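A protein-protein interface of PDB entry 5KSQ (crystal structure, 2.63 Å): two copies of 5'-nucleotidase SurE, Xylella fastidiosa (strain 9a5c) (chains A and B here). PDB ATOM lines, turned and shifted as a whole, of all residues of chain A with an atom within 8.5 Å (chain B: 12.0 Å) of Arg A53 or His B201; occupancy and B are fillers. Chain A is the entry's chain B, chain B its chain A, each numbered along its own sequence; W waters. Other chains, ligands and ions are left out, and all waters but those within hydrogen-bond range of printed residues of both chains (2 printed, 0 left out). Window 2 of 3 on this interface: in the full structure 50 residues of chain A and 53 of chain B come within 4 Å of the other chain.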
ATOM      1  N   ALA A  34      -5.735 -23.480 -10.021  1.00  0.00           N
ATOM      2  CA  ALA A  34      -6.708 -22.937 -10.968  1.00  0.00           C
ATOM      3  C   ALA A  34      -8.050 -22.597 -10.311  1.00  0.00           C
ATOM      4  O   ALA A  34      -8.402 -23.175  -9.283  1.00  0.00           O
ATOM      5  CB  ALA A  34      -6.911 -23.920 -12.121  1.00  0.00           C
ATOM      6  N   ASP A  36     -12.159 -22.302  -9.556  1.00  0.00           N
ATOM      7  CA  ASP A  36     -13.146 -23.365  -9.384  1.00  0.00           C
ATOM      8  C   ASP A  36     -14.153 -23.419 -10.531  1.00  0.00           C
ATOM      9  O   ASP A  36     -14.777 -24.454 -10.768  1.00  0.00           O
ATOM     10  CB  ASP A  36     -13.872 -23.220  -8.042  1.00  0.00           C
ATOM     11  CG  ASP A  36     -14.585 -21.890  -7.903  1.00  0.00           C
ATOM     12  OD1 ASP A  36     -14.114 -20.894  -8.492  1.00  0.00           O
ATOM     13  OD2 ASP A  36     -15.618 -21.838  -7.202  1.00  0.00           O
ATOM     14  N   THR A  50     -12.022  -8.963   1.073  1.00  0.00           N
ATOM     15  CA  THR A  50     -12.523 -10.171   1.726  1.00  0.00           C
ATOM     16  C   THR A  50     -11.489 -11.296   1.684  1.00  0.00           C
ATOM     17  O   THR A  50     -10.642 -11.326   0.792  1.00  0.00           O
ATOM     18  CB  THR A  50     -13.846 -10.655   1.081  1.00  0.00           C
ATOM     19  OG1 THR A  50     -13.675 -10.783  -0.337  1.00  0.00           O
ATOM     20  CG2 THR A  50     -14.974  -9.674   1.365  1.00  0.00           C
ATOM     21  N   PRO A  51     -11.545 -12.218   2.662  1.00  0.00           N
ATOM     22  CA  PRO A  51     -10.656 -13.387   2.659  1.00  0.00           C
ATOM     23  C   PRO A  51     -11.041 -14.385   1.566  1.00  0.00           C
ATOM     24  O   PRO A  51     -12.169 -14.344   1.077  1.00  0.00           O
ATOM     25  CB  PRO A  51     -10.884 -14.000   4.043  1.00  0.00           C
ATOM     26  CG  PRO A  51     -12.253 -13.558   4.429  1.00  0.00           C
ATOM     27  CD  PRO A  51     -12.393 -12.176   3.867  1.00  0.00           C
ATOM     28  N   ILE A  52     -10.117 -15.270   1.200  1.00  0.00           N
ATOM     29  CA  ILE A  52     -10.327 -16.193   0.084  1.00  0.00           C
ATOM     30  C   ILE A  52     -10.303 -17.661   0.519  1.00  0.00           C
ATOM     31  O   ILE A  52      -9.449 -18.072   1.303  1.00  0.00           O
ATOM     32  CB  ILE A  52      -9.264 -15.983  -1.017  1.00  0.00           C
ATOM     33  CG1 ILE A  52      -9.122 -14.496  -1.353  1.00  0.00           C
ATOM     34  CG2 ILE A  52      -9.609 -16.787  -2.261  1.00  0.00           C
ATOM     35  CD1 ILE A  52      -7.984 -14.194  -2.304  1.00  0.00           C
ATOM     36  N   ARG A  53     -11.243 -18.445  -0.006  1.00  0.00           N
ATOM     37  CA  ARG A  53     -11.327 -19.874   0.290  1.00  0.00           C
ATOM     38  C   ARG A  53     -10.457 -20.694  -0.663  1.00  0.00           C
ATOM     39  O   ARG A  53     -10.181 -20.272  -1.785  1.00  0.00           O
ATOM     40  CB  ARG A  53     -12.781 -20.349   0.189  1.00  0.00           C
ATOM     41  CG  ARG A  53     -13.304 -21.066   1.424  1.00  0.00           C
ATOM     42  CD  ARG A  53     -13.848 -20.082   2.448  1.00  0.00           C
ATOM     43  NE  ARG A  53     -14.422 -20.761   3.607  1.00  0.00           N
ATOM     44  CZ  ARG A  53     -15.107 -20.152   4.570  1.00  0.00           C
ATOM     45  NH1 ARG A  53     -15.313 -18.843   4.516  1.00  0.00           N
ATOM     46  NH2 ARG A  53     -15.591 -20.853   5.587  1.00  0.00           N
ATOM     47  N   ALA A  54     -10.033 -21.871  -0.212  1.00  0.00           N
ATOM     48  CA  ALA A  54      -9.221 -22.768  -1.033  1.00  0.00           C
ATOM     49  C   ALA A  54      -9.304 -24.210  -0.537  1.00  0.00           C
ATOM     50  O   ALA A  54      -9.418 -24.454   0.664  1.00  0.00           O
ATOM     51  CB  ALA A  54      -7.772 -22.301  -1.059  1.00  0.00           C
ATOM     52  N   LYS A  55      -9.249 -25.161  -1.465  1.00  0.00           N
ATOM     53  CA  LYS A  55      -9.280 -26.576  -1.107  1.00  0.00           C
ATOM     54  C   LYS A  55      -8.369 -27.408  -2.006  1.00  0.00           C
ATOM     55  O   LYS A  55      -8.049 -27.009  -3.125  1.00  0.00           O
ATOM     56  CB  LYS A  55     -10.709 -27.123  -1.157  1.00  0.00           C
ATOM     57  CG  LYS A  55     -11.291 -27.229  -2.556  1.00  0.00           C
ATOM     58  N   GLN A  56      -7.962 -28.570  -1.507  1.00  0.00           N
ATOM     59  CA  GLN A  56      -7.060 -29.451  -2.238  1.00  0.00           C
ATOM     60  C   GLN A  56      -7.813 -30.579  -2.941  1.00  0.00           C
ATOM     61  O   GLN A  56      -8.680 -31.222  -2.350  1.00  0.00           O
ATOM     62  CB  GLN A  56      -6.009 -30.033  -1.290  1.00  0.00           C
ATOM     63  CG  GLN A  56      -5.141 -31.114  -1.907  1.00  0.00           C
ATOM     64  CD  GLN A  56      -4.061 -31.604  -0.963  1.00  0.00           C
ATOM     65  OE1 GLN A  56      -3.730 -30.939   0.019  1.00  0.00           O
ATOM     66  NE2 GLN A  56      -3.508 -32.776  -1.255  1.00  0.00           N
ATOM     67  N   TYR A  62      -4.720 -27.806  -6.718  1.00  0.00           N
ATOM     68  CA  TYR A  62      -5.440 -26.959  -5.769  1.00  0.00           C
ATOM     69  C   TYR A  62      -6.557 -26.169  -6.453  1.00  0.00           C
ATOM     70  O   TYR A  62      -6.376 -25.646  -7.554  1.00  0.00           O
ATOM     71  CB  TYR A  62      -4.479 -25.996  -5.067  1.00  0.00           C
ATOM     72  CG  TYR A  62      -3.746 -26.595  -3.888  1.00  0.00           C
ATOM     73  CD1 TYR A  62      -2.576 -27.323  -4.066  1.00  0.00           C
ATOM     74  CD2 TYR A  62      -4.220 -26.422  -2.594  1.00  0.00           C
ATOM     75  CE1 TYR A  62      -1.904 -27.867  -2.988  1.00  0.00           C
ATOM     76  CE2 TYR A  62      -3.553 -26.963  -1.509  1.00  0.00           C
ATOM     77  CZ  TYR A  62      -2.396 -27.684  -1.712  1.00  0.00           C
ATOM     78  OH  TYR A  62      -1.729 -28.223  -0.638  1.00  0.00           O
ATOM     79  N   SER A  63      -7.706 -26.082  -5.789  1.00  0.00           N
ATOM     80  CA  SER A  63      -8.852 -25.338  -6.309  1.00  0.00           C
ATOM     81  C   SER A  63      -9.052 -24.032  -5.542  1.00  0.00           C
ATOM     82  O   SER A  63      -9.109 -24.030  -4.311  1.00  0.00           O
ATOM     83  CB  SER A  63     -10.119 -26.192  -6.233  1.00  0.00           C
ATOM     84  OG  SER A  63     -11.259 -25.457  -6.645  1.00  0.00           O
ATOM     85  N   VAL A  64      -9.162 -22.927  -6.274  1.00  0.00           N
ATOM     86  CA  VAL A  64      -9.274 -21.604  -5.665  1.00  0.00           C
ATOM     87  C   VAL A  64     -10.541 -20.876  -6.111  1.00  0.00           C
ATOM     88  O   VAL A  64     -10.850 -20.823  -7.301  1.00  0.00           O
ATOM     89  CB  VAL A  64      -8.044 -20.731  -5.995  1.00  0.00           C
ATOM     90  CG1 VAL A  64      -8.232 -19.310  -5.477  1.00  0.00           C
ATOM     91  CG2 VAL A  64      -6.778 -21.352  -5.420  1.00  0.00           C
ATOM     92  N   ALA A  65     -11.271 -20.319  -5.149  1.00  0.00           N
ATOM     93  CA  ALA A  65     -12.484 -19.565  -5.444  1.00  0.00           C
ATOM     94  C   ALA A  65     -12.190 -18.072  -5.604  1.00  0.00           C
ATOM     95  O   ALA A  65     -12.503 -17.271  -4.721  1.00  0.00           O
ATOM     96  CB  ALA A  65     -13.522 -19.791  -4.355  1.00  0.00           C
ATOM     97  N   GLY A  66     -11.592 -17.706  -6.734  1.00  0.00           N
ATOM     98  CA  GLY A  66     -11.249 -16.319  -7.001  1.00  0.00           C
ATOM     99  C   GLY A  66     -10.718 -16.093  -8.404  1.00  0.00           C
ATOM    100  O   GLY A  66     -10.792 -16.977  -9.257  1.00  0.00           O
ATOM    101  N   ASP A  70      -5.381 -14.008  -8.366  1.00  0.00           N
ATOM    102  CA  ASP A  70      -5.320 -14.452  -6.978  1.00  0.00           C
ATOM    103  C   ASP A  70      -4.623 -15.805  -6.869  1.00  0.00           C
ATOM    104  O   ASP A  70      -3.925 -16.073  -5.891  1.00  0.00           O
ATOM    105  CB  ASP A  70      -6.723 -14.541  -6.368  1.00  0.00           C
ATOM    106  CG  ASP A  70      -7.394 -13.186  -6.235  1.00  0.00           C
ATOM    107  OD1 ASP A  70      -6.676 -12.174  -6.091  1.00  0.00           O
ATOM    108  OD2 ASP A  70      -8.642 -13.137  -6.267  1.00  0.00           O
ATOM    109  N   CYS A  71      -4.817 -16.653  -7.876  1.00  0.00           N
ATOM    110  CA  CYS A  71      -4.232 -17.991  -7.877  1.00  0.00           C
ATOM    111  C   CYS A  71      -2.703 -17.961  -7.885  1.00  0.00           C
ATOM    112  O   CYS A  71      -2.058 -18.585  -7.044  1.00  0.00           O
ATOM    113  CB  CYS A  71      -4.746 -18.803  -9.068  1.00  0.00           C
ATOM    114  SG  CYS A  71      -6.509 -19.212  -9.000  1.00  0.00           S
ATOM    115  N   LEU A  74      -1.034 -15.995  -4.603  1.00  0.00           N
ATOM    116  CA  LEU A  74      -1.032 -16.787  -3.376  1.00  0.00           C
ATOM    117  C   LEU A  74      -0.026 -17.931  -3.434  1.00  0.00           C
ATOM    118  O   LEU A  74       0.639 -18.234  -2.444  1.00  0.00           O
ATOM    119  CB  LEU A  74      -2.431 -17.340  -3.089  1.00  0.00           C
ATOM    120  CG  LEU A  74      -3.509 -16.347  -2.649  1.00  0.00           C
ATOM    121  CD1 LEU A  74      -4.843 -17.055  -2.463  1.00  0.00           C
ATOM    122  CD2 LEU A  74      -3.097 -15.635  -1.370  1.00  0.00           C
ATOM    123  N   LEU A  79       1.314 -20.034   0.012  1.00  0.00           N
ATOM    124  CA  LEU A  79       0.324 -21.104  -0.084  1.00  0.00           C
ATOM    125  C   LEU A  79       0.992 -22.469  -0.212  1.00  0.00           C
ATOM    126  O   LEU A  79       0.476 -23.473   0.280  1.00  0.00           O
ATOM    127  CB  LEU A  79      -0.622 -20.869  -1.265  1.00  0.00           C
ATOM    128  CG  LEU A  79      -1.739 -21.896  -1.472  1.00  0.00           C
ATOM    129  CD1 LEU A  79      -2.681 -21.918  -0.278  1.00  0.00           C
ATOM    130  CD2 LEU A  79      -2.505 -21.620  -2.756  1.00  0.00           C
ATOM    131  N   CYS B 192       1.296 -13.896   2.365  1.00  0.00           N
ATOM    132  CA  CYS B 192       0.002 -14.525   2.602  1.00  0.00           C
ATOM    133  C   CYS B 192      -0.218 -14.772   4.092  1.00  0.00           C
ATOM    134  O   CYS B 192       0.673 -15.260   4.785  1.00  0.00           O
ATOM    135  CB  CYS B 192      -0.086 -15.841   1.825  1.00  0.00           C
ATOM    136  SG  CYS B 192      -1.505 -16.883   2.225  1.00  0.00           S
ATOM    137  N   LEU B 193      -1.407 -14.431   4.580  1.00  0.00           N
ATOM    138  CA  LEU B 193      -1.734 -14.598   5.994  1.00  0.00           C
ATOM    139  C   LEU B 193      -2.792 -15.681   6.197  1.00  0.00           C
ATOM    140  O   LEU B 193      -3.704 -15.830   5.386  1.00  0.00           O
ATOM    141  CB  LEU B 193      -2.221 -13.274   6.588  1.00  0.00           C
ATOM    142  CG  LEU B 193      -1.282 -12.077   6.427  1.00  0.00           C
ATOM    143  CD1 LEU B 193      -1.896 -10.825   7.036  1.00  0.00           C
ATOM    144  CD2 LEU B 193       0.075 -12.369   7.045  1.00  0.00           C
ATOM    145  N   THR B 194      -2.666 -16.427   7.290  1.00  0.00           N
ATOM    146  CA  THR B 194      -3.580 -17.529   7.578  1.00  0.00           C
ATOM    147  C   THR B 194      -4.402 -17.272   8.839  1.00  0.00           C
ATOM    148  O   THR B 194      -3.848 -17.063   9.918  1.00  0.00           O
ATOM    149  CB  THR B 194      -2.817 -18.860   7.741  1.00  0.00           C
ATOM    150  OG1 THR B 194      -2.087 -19.149   6.543  1.00  0.00           O
ATOM    151  CG2 THR B 194      -3.782 -20.000   8.028  1.00  0.00           C
ATOM    152  N   GLN B 195      -5.725 -17.294   8.697  1.00  0.00           N
ATOM    153  CA  GLN B 195      -6.627 -17.101   9.830  1.00  0.00           C
ATOM    154  C   GLN B 195      -7.754 -18.131   9.831  1.00  0.00           C
ATOM    155  O   GLN B 195      -7.814 -19.002   8.965  1.00  0.00           O
ATOM    156  CB  GLN B 195      -7.215 -15.687   9.822  1.00  0.00           C
ATOM    157  CG  GLN B 195      -6.200 -14.584  10.075  1.00  0.00           C
ATOM    158  CD  GLN B 195      -6.840 -13.212  10.153  1.00  0.00           C
ATOM    159  OE1 GLN B 195      -8.053 -13.071   9.997  1.00  0.00           O
ATOM    160  NE2 GLN B 195      -6.026 -12.192  10.400  1.00  0.00           N
ATOM    161  N   THR B 196      -8.645 -18.024  10.813  1.00  0.00           N
ATOM    162  CA  THR B 196      -9.783 -18.930  10.921  1.00  0.00           C
ATOM    163  C   THR B 196     -11.099 -18.166  11.032  1.00  0.00           C
ATOM    164  O   THR B 196     -11.175 -17.132  11.695  1.00  0.00           O
ATOM    165  CB  THR B 196      -9.647 -19.871  12.135  1.00  0.00           C
ATOM    166  OG1 THR B 196      -9.510 -19.094  13.331  1.00  0.00           O
ATOM    167  CG2 THR B 196      -8.434 -20.777  11.979  1.00  0.00           C
ATOM    168  N   ASP B 197     -12.133 -18.685  10.377  1.00  0.00           N
ATOM    169  CA  ASP B 197     -13.458 -18.080  10.428  1.00  0.00           C
ATOM    170  C   ASP B 197     -14.169 -18.507  11.715  1.00  0.00           C
ATOM    171  O   ASP B 197     -13.738 -19.457  12.368  1.00  0.00           O
ATOM    172  CB  ASP B 197     -14.270 -18.474   9.185  1.00  0.00           C
ATOM    173  CG  ASP B 197     -14.693 -19.930   9.196  1.00  0.00           C
ATOM    174  OD1 ASP B 197     -13.997 -20.755   9.823  1.00  0.00           O
ATOM    175  OD2 ASP B 197     -15.725 -20.250   8.570  1.00  0.00           O
ATOM    176  N   PRO B 198     -15.251 -17.801  12.094  1.00  0.00           N
ATOM    177  CA  PRO B 198     -16.002 -18.158  13.306  1.00  0.00           C
ATOM    178  C   PRO B 198     -16.565 -19.583  13.320  1.00  0.00           C
ATOM    179  O   PRO B 198     -17.102 -20.006  14.344  1.00  0.00           O
ATOM    180  CB  PRO B 198     -17.152 -17.147  13.307  1.00  0.00           C
ATOM    181  CG  PRO B 198     -16.599 -15.965  12.605  1.00  0.00           C
ATOM    182  CD  PRO B 198     -15.704 -16.515  11.532  1.00  0.00           C
ATOM    183  N   ARG B 199     -16.446 -20.309  12.212  1.00  0.00           N
ATOM    184  CA  ARG B 199     -16.971 -21.668  12.135  1.00  0.00           C
ATOM    185  C   ARG B 199     -15.873 -22.729  12.235  1.00  0.00           C
ATOM    186  O   ARG B 199     -16.155 -23.900  12.492  1.00  0.00           O
ATOM    187  CB  ARG B 199     -17.792 -21.855  10.858  1.00  0.00           C
ATOM    188  CG  ARG B 199     -18.923 -20.848  10.715  1.00  0.00           C
ATOM    189  CD  ARG B 199     -19.796 -21.141   9.507  1.00  0.00           C
ATOM    190  NE  ARG B 199     -20.807 -20.107   9.310  1.00  0.00           N
ATOM    191  CZ  ARG B 199     -21.989 -20.091   9.919  1.00  0.00           C
ATOM    192  NH1 ARG B 199     -22.314 -21.055  10.769  1.00  0.00           N
ATOM    193  NH2 ARG B 199     -22.848 -19.109   9.678  1.00  0.00           N
ATOM    194  N   GLY B 200     -14.625 -22.318  12.031  1.00  0.00           N
ATOM    195  CA  GLY B 200     -13.495 -23.217  12.196  1.00  0.00           C
ATOM    196  C   GLY B 200     -12.697 -23.484  10.934  1.00  0.00           C
ATOM    197  O   GLY B 200     -11.613 -24.064  10.991  1.00  0.00           O
ATOM    198  N   HIS B 201     -13.229 -23.062   9.792  1.00  0.00           N
ATOM    199  CA  HIS B 201     -12.567 -23.283   8.509  1.00  0.00           C
ATOM    200  C   HIS B 201     -11.315 -22.419   8.370  1.00  0.00           C
ATOM    201  O   HIS B 201     -11.045 -21.561   9.210  1.00  0.00           O
ATOM    202  CB  HIS B 201     -13.532 -23.004   7.354  1.00  0.00           C
ATOM    203  CG  HIS B 201     -14.780 -23.830   7.394  1.00  0.00           C
ATOM    204  ND1 HIS B 201     -15.756 -23.660   8.352  1.00  0.00           N
ATOM    205  CD2 HIS B 201     -15.212 -24.833   6.591  1.00  0.00           C
ATOM    206  CE1 HIS B 201     -16.734 -24.522   8.139  1.00  0.00           C
ATOM    207  NE2 HIS B 201     -16.428 -25.245   7.077  1.00  0.00           N
ATOM    208  N   THR B 202     -10.554 -22.651   7.303  1.00  0.00           N
ATOM    209  CA  THR B 202      -9.320 -21.910   7.064  1.00  0.00           C
ATOM    210  C   THR B 202      -9.480 -20.917   5.915  1.00  0.00           C
ATOM    211  O   THR B 202      -9.956 -21.274   4.838  1.00  0.00           O
ATOM    212  CB  THR B 202      -8.145 -22.862   6.755  1.00  0.00           C
ATOM    213  OG1 THR B 202      -8.012 -23.821   7.811  1.00  0.00           O
ATOM    214  CG2 THR B 202      -6.845 -22.084   6.614  1.00  0.00           C
ATOM    215  N   ILE B 203      -9.082 -19.671   6.154  1.00  0.00           N
ATOM    216  CA  ILE B 203      -9.185 -18.618   5.146  1.00  0.00           C
ATOM    217  C   ILE B 203      -7.836 -17.941   4.906  1.00  0.00           C
ATOM    218  O   ILE B 203      -6.920 -18.068   5.716  1.00  0.00           O
ATOM    219  CB  ILE B 203     -10.225 -17.555   5.550  1.00  0.00           C
ATOM    220  CG1 ILE B 203      -9.877 -16.961   6.917  1.00  0.00           C
ATOM    221  CG2 ILE B 203     -11.621 -18.158   5.576  1.00  0.00           C
ATOM    222  CD1 ILE B 203     -10.888 -15.955   7.423  1.00  0.00           C
ATOM    223  N   TYR B 204      -7.719 -17.225   3.792  1.00  0.00           N
ATOM    224  CA  TYR B 204      -6.466 -16.557   3.441  1.00  0.00           C
ATOM    225  C   TYR B 204      -6.665 -15.089   3.064  1.00  0.00           C
ATOM    226  O   TYR B 204      -7.478 -14.764   2.201  1.00  0.00           O
ATOM    227  CB  TYR B 204      -5.767 -17.290   2.291  1.00  0.00           C
ATOM    228  CG  TYR B 204      -5.422 -18.733   2.584  1.00  0.00           C
ATOM    229  CD1 TYR B 204      -4.279 -19.062   3.301  1.00  0.00           C
ATOM    230  CD2 TYR B 204      -6.233 -19.767   2.136  1.00  0.00           C
ATOM    231  CE1 TYR B 204      -3.957 -20.379   3.569  1.00  0.00           C
ATOM    232  CE2 TYR B 204      -5.920 -21.087   2.398  1.00  0.00           C
ATOM    233  CZ  TYR B 204      -4.781 -21.387   3.115  1.00  0.00           C
ATOM    234  OH  TYR B 204      -4.464 -22.700   3.379  1.00  0.00           O
ATOM    235  N   TRP B 205      -5.910 -14.209   3.717  1.00  0.00           N
ATOM    236  CA  TRP B 205      -5.907 -12.790   3.381  1.00  0.00           C
ATOM    237  C   TRP B 205      -4.690 -12.453   2.527  1.00  0.00           C
ATOM    238  O   TRP B 205      -3.649 -13.102   2.631  1.00  0.00           O
ATOM    239  CB  TRP B 205      -5.858 -11.932   4.647  1.00  0.00           C
ATOM    240  CG  TRP B 205      -7.141 -11.847   5.419  1.00  0.00           C
ATOM    241  CD1 TRP B 205      -7.513 -12.622   6.477  1.00  0.00           C
ATOM    242  CD2 TRP B 205      -8.208 -10.913   5.210  1.00  0.00           C
ATOM    243  NE1 TRP B 205      -8.751 -12.237   6.934  1.00  0.00           N
ATOM    244  CE2 TRP B 205      -9.199 -11.190   6.172  1.00  0.00           C
ATOM    245  CE3 TRP B 205      -8.425  -9.875   4.298  1.00  0.00           C
ATOM    246  CZ2 TRP B 205     -10.388 -10.467   6.250  1.00  0.00           C
ATOM    247  CZ3 TRP B 205      -9.606  -9.158   4.375  1.00  0.00           C
ATOM    248  CH2 TRP B 205     -10.573  -9.457   5.345  1.00  0.00           C
ATOM    249  N   ILE B 206      -4.823 -11.434   1.684  1.00  0.00           N
ATOM    250  CA  ILE B 206      -3.672 -10.873   0.988  1.00  0.00           C
ATOM    251  C   ILE B 206      -3.137  -9.701   1.802  1.00  0.00           C
ATOM    252  O   ILE B 206      -3.823  -8.690   1.971  1.00  0.00           O
ATOM    253  CB  ILE B 206      -4.022 -10.409  -0.437  1.00  0.00           C
ATOM    254  CG1 ILE B 206      -4.368 -11.612  -1.316  1.00  0.00           C
ATOM    255  CG2 ILE B 206      -2.864  -9.628  -1.041  1.00  0.00           C
ATOM    256  CD1 ILE B 206      -4.539 -11.274  -2.780  1.00  0.00           C
HETATM  257  O   HOH W   1      -7.726 -10.398   0.918  1.00  0.00           O
HETATM  258  O   HOH W   2      -9.541 -22.319   2.594  1.00  0.00           O
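Water W2 bridges the backbone carbonyl oxygen (O) of Thr B202 (2.5 Å) and the backbone carbonyl oxygen (O) of Ala A54 (2.9 Å). Water W1 lies within hydrogen-bond range of the backbone carbonyl oxygen (O) of Thr A50 (3.1 Å) and the backbone NH (N) of Ile B206 (3.2 Å).
No position is printed for both chains.
C of Thr A50 touches CZ3 of Trp B205 (3.9 Å). CB of Pro A51 touches CD1 of Ile B203, 3.9 Å away. Pro A51 touches Tyr B204 (CA to O, 3.5 Å). Trp B205 touches Pro A51. Ile A52 touches Ile B203. His B201 touches Arg A53 (CB to NH2, 3.5 Å). Ile B203 touches Arg A53 (CG2 to NH1, 3.9 Å).
O of Leu B193 lies within hydrogen-bond range of N of Trp B205, at 3.2 Å. The backbone NH (N) of Ile B203 lies within hydrogen-bond range of the backbone carbonyl oxygen (O) of Gln B195 (3.2 Å). The side-chain amide oxygen (OE1) of Gln B195 is in hydrogen-bond range of the indole nitrogen (NE1) of Trp B205 (3.3 Å). The side-chain carboxylate (OD1) of Asp B197 sits close to the backbone NH (N) of Arg B199, 3.5 Å away. The side-chain carboxylate (OD1) of Asp B197 is in hydrogen-bond range of the backbone NH (N) of Gly B200 (2.8 Å). OD1 of Asp B197 sits at hydrogen-bond distance from N of His B201.
Along chain B the printed residues that touch a printed residue of chain A span positions 197 to 205. Among the printed residues, Asp or Glu carboxylates within 4 Å of a Lys or Arg side-chain nitrogen of the other chain: Arg A53 with Asp B197 (3.0 Å).
Of the printed residues of chain B, Thr A50 touches Trp B205. Pro A51 touches just these residues of chain B: Ile B203, Tyr B204 and Trp B205. Arg A53 touches three residues of chain B. Val A64 touches none of the printed residues of chain B. Ala A65 touches none of the printed residues of chain B. Cys B192 touches none of the printed residues of chain A. Of the printed residues of chain A, Asp B197 touches Arg A53 (3.0 Å). No residue of chain A comes within 4 Å of Gly B200. Thr B202 touches none of the printed residues of chain A. Of the printed residues of chain A, Ile B203 touches Pro A51 (3.9 Å), Ile A52 (3.9 Å) and Arg A53 (3.9 Å). Printed residues of chain A within 4 Å of Tyr B204: Pro A51 (3.5 Å) and Ile A52 (2.9 Å). Of the printed residues of chain A, Trp B205 touches Thr A50 and Pro A51. The nearest residue of chain A that does not touch His B201 is Ala A54 (8.0 Å).
The guanidinium group (NH2) of Arg A53 lies within salt-bridge range of the side-chain carboxylate (OD2) of Asp B197, at 3.0 Å. O of Tyr B204 lies within hydrogen-bond range of N of Ile A52.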
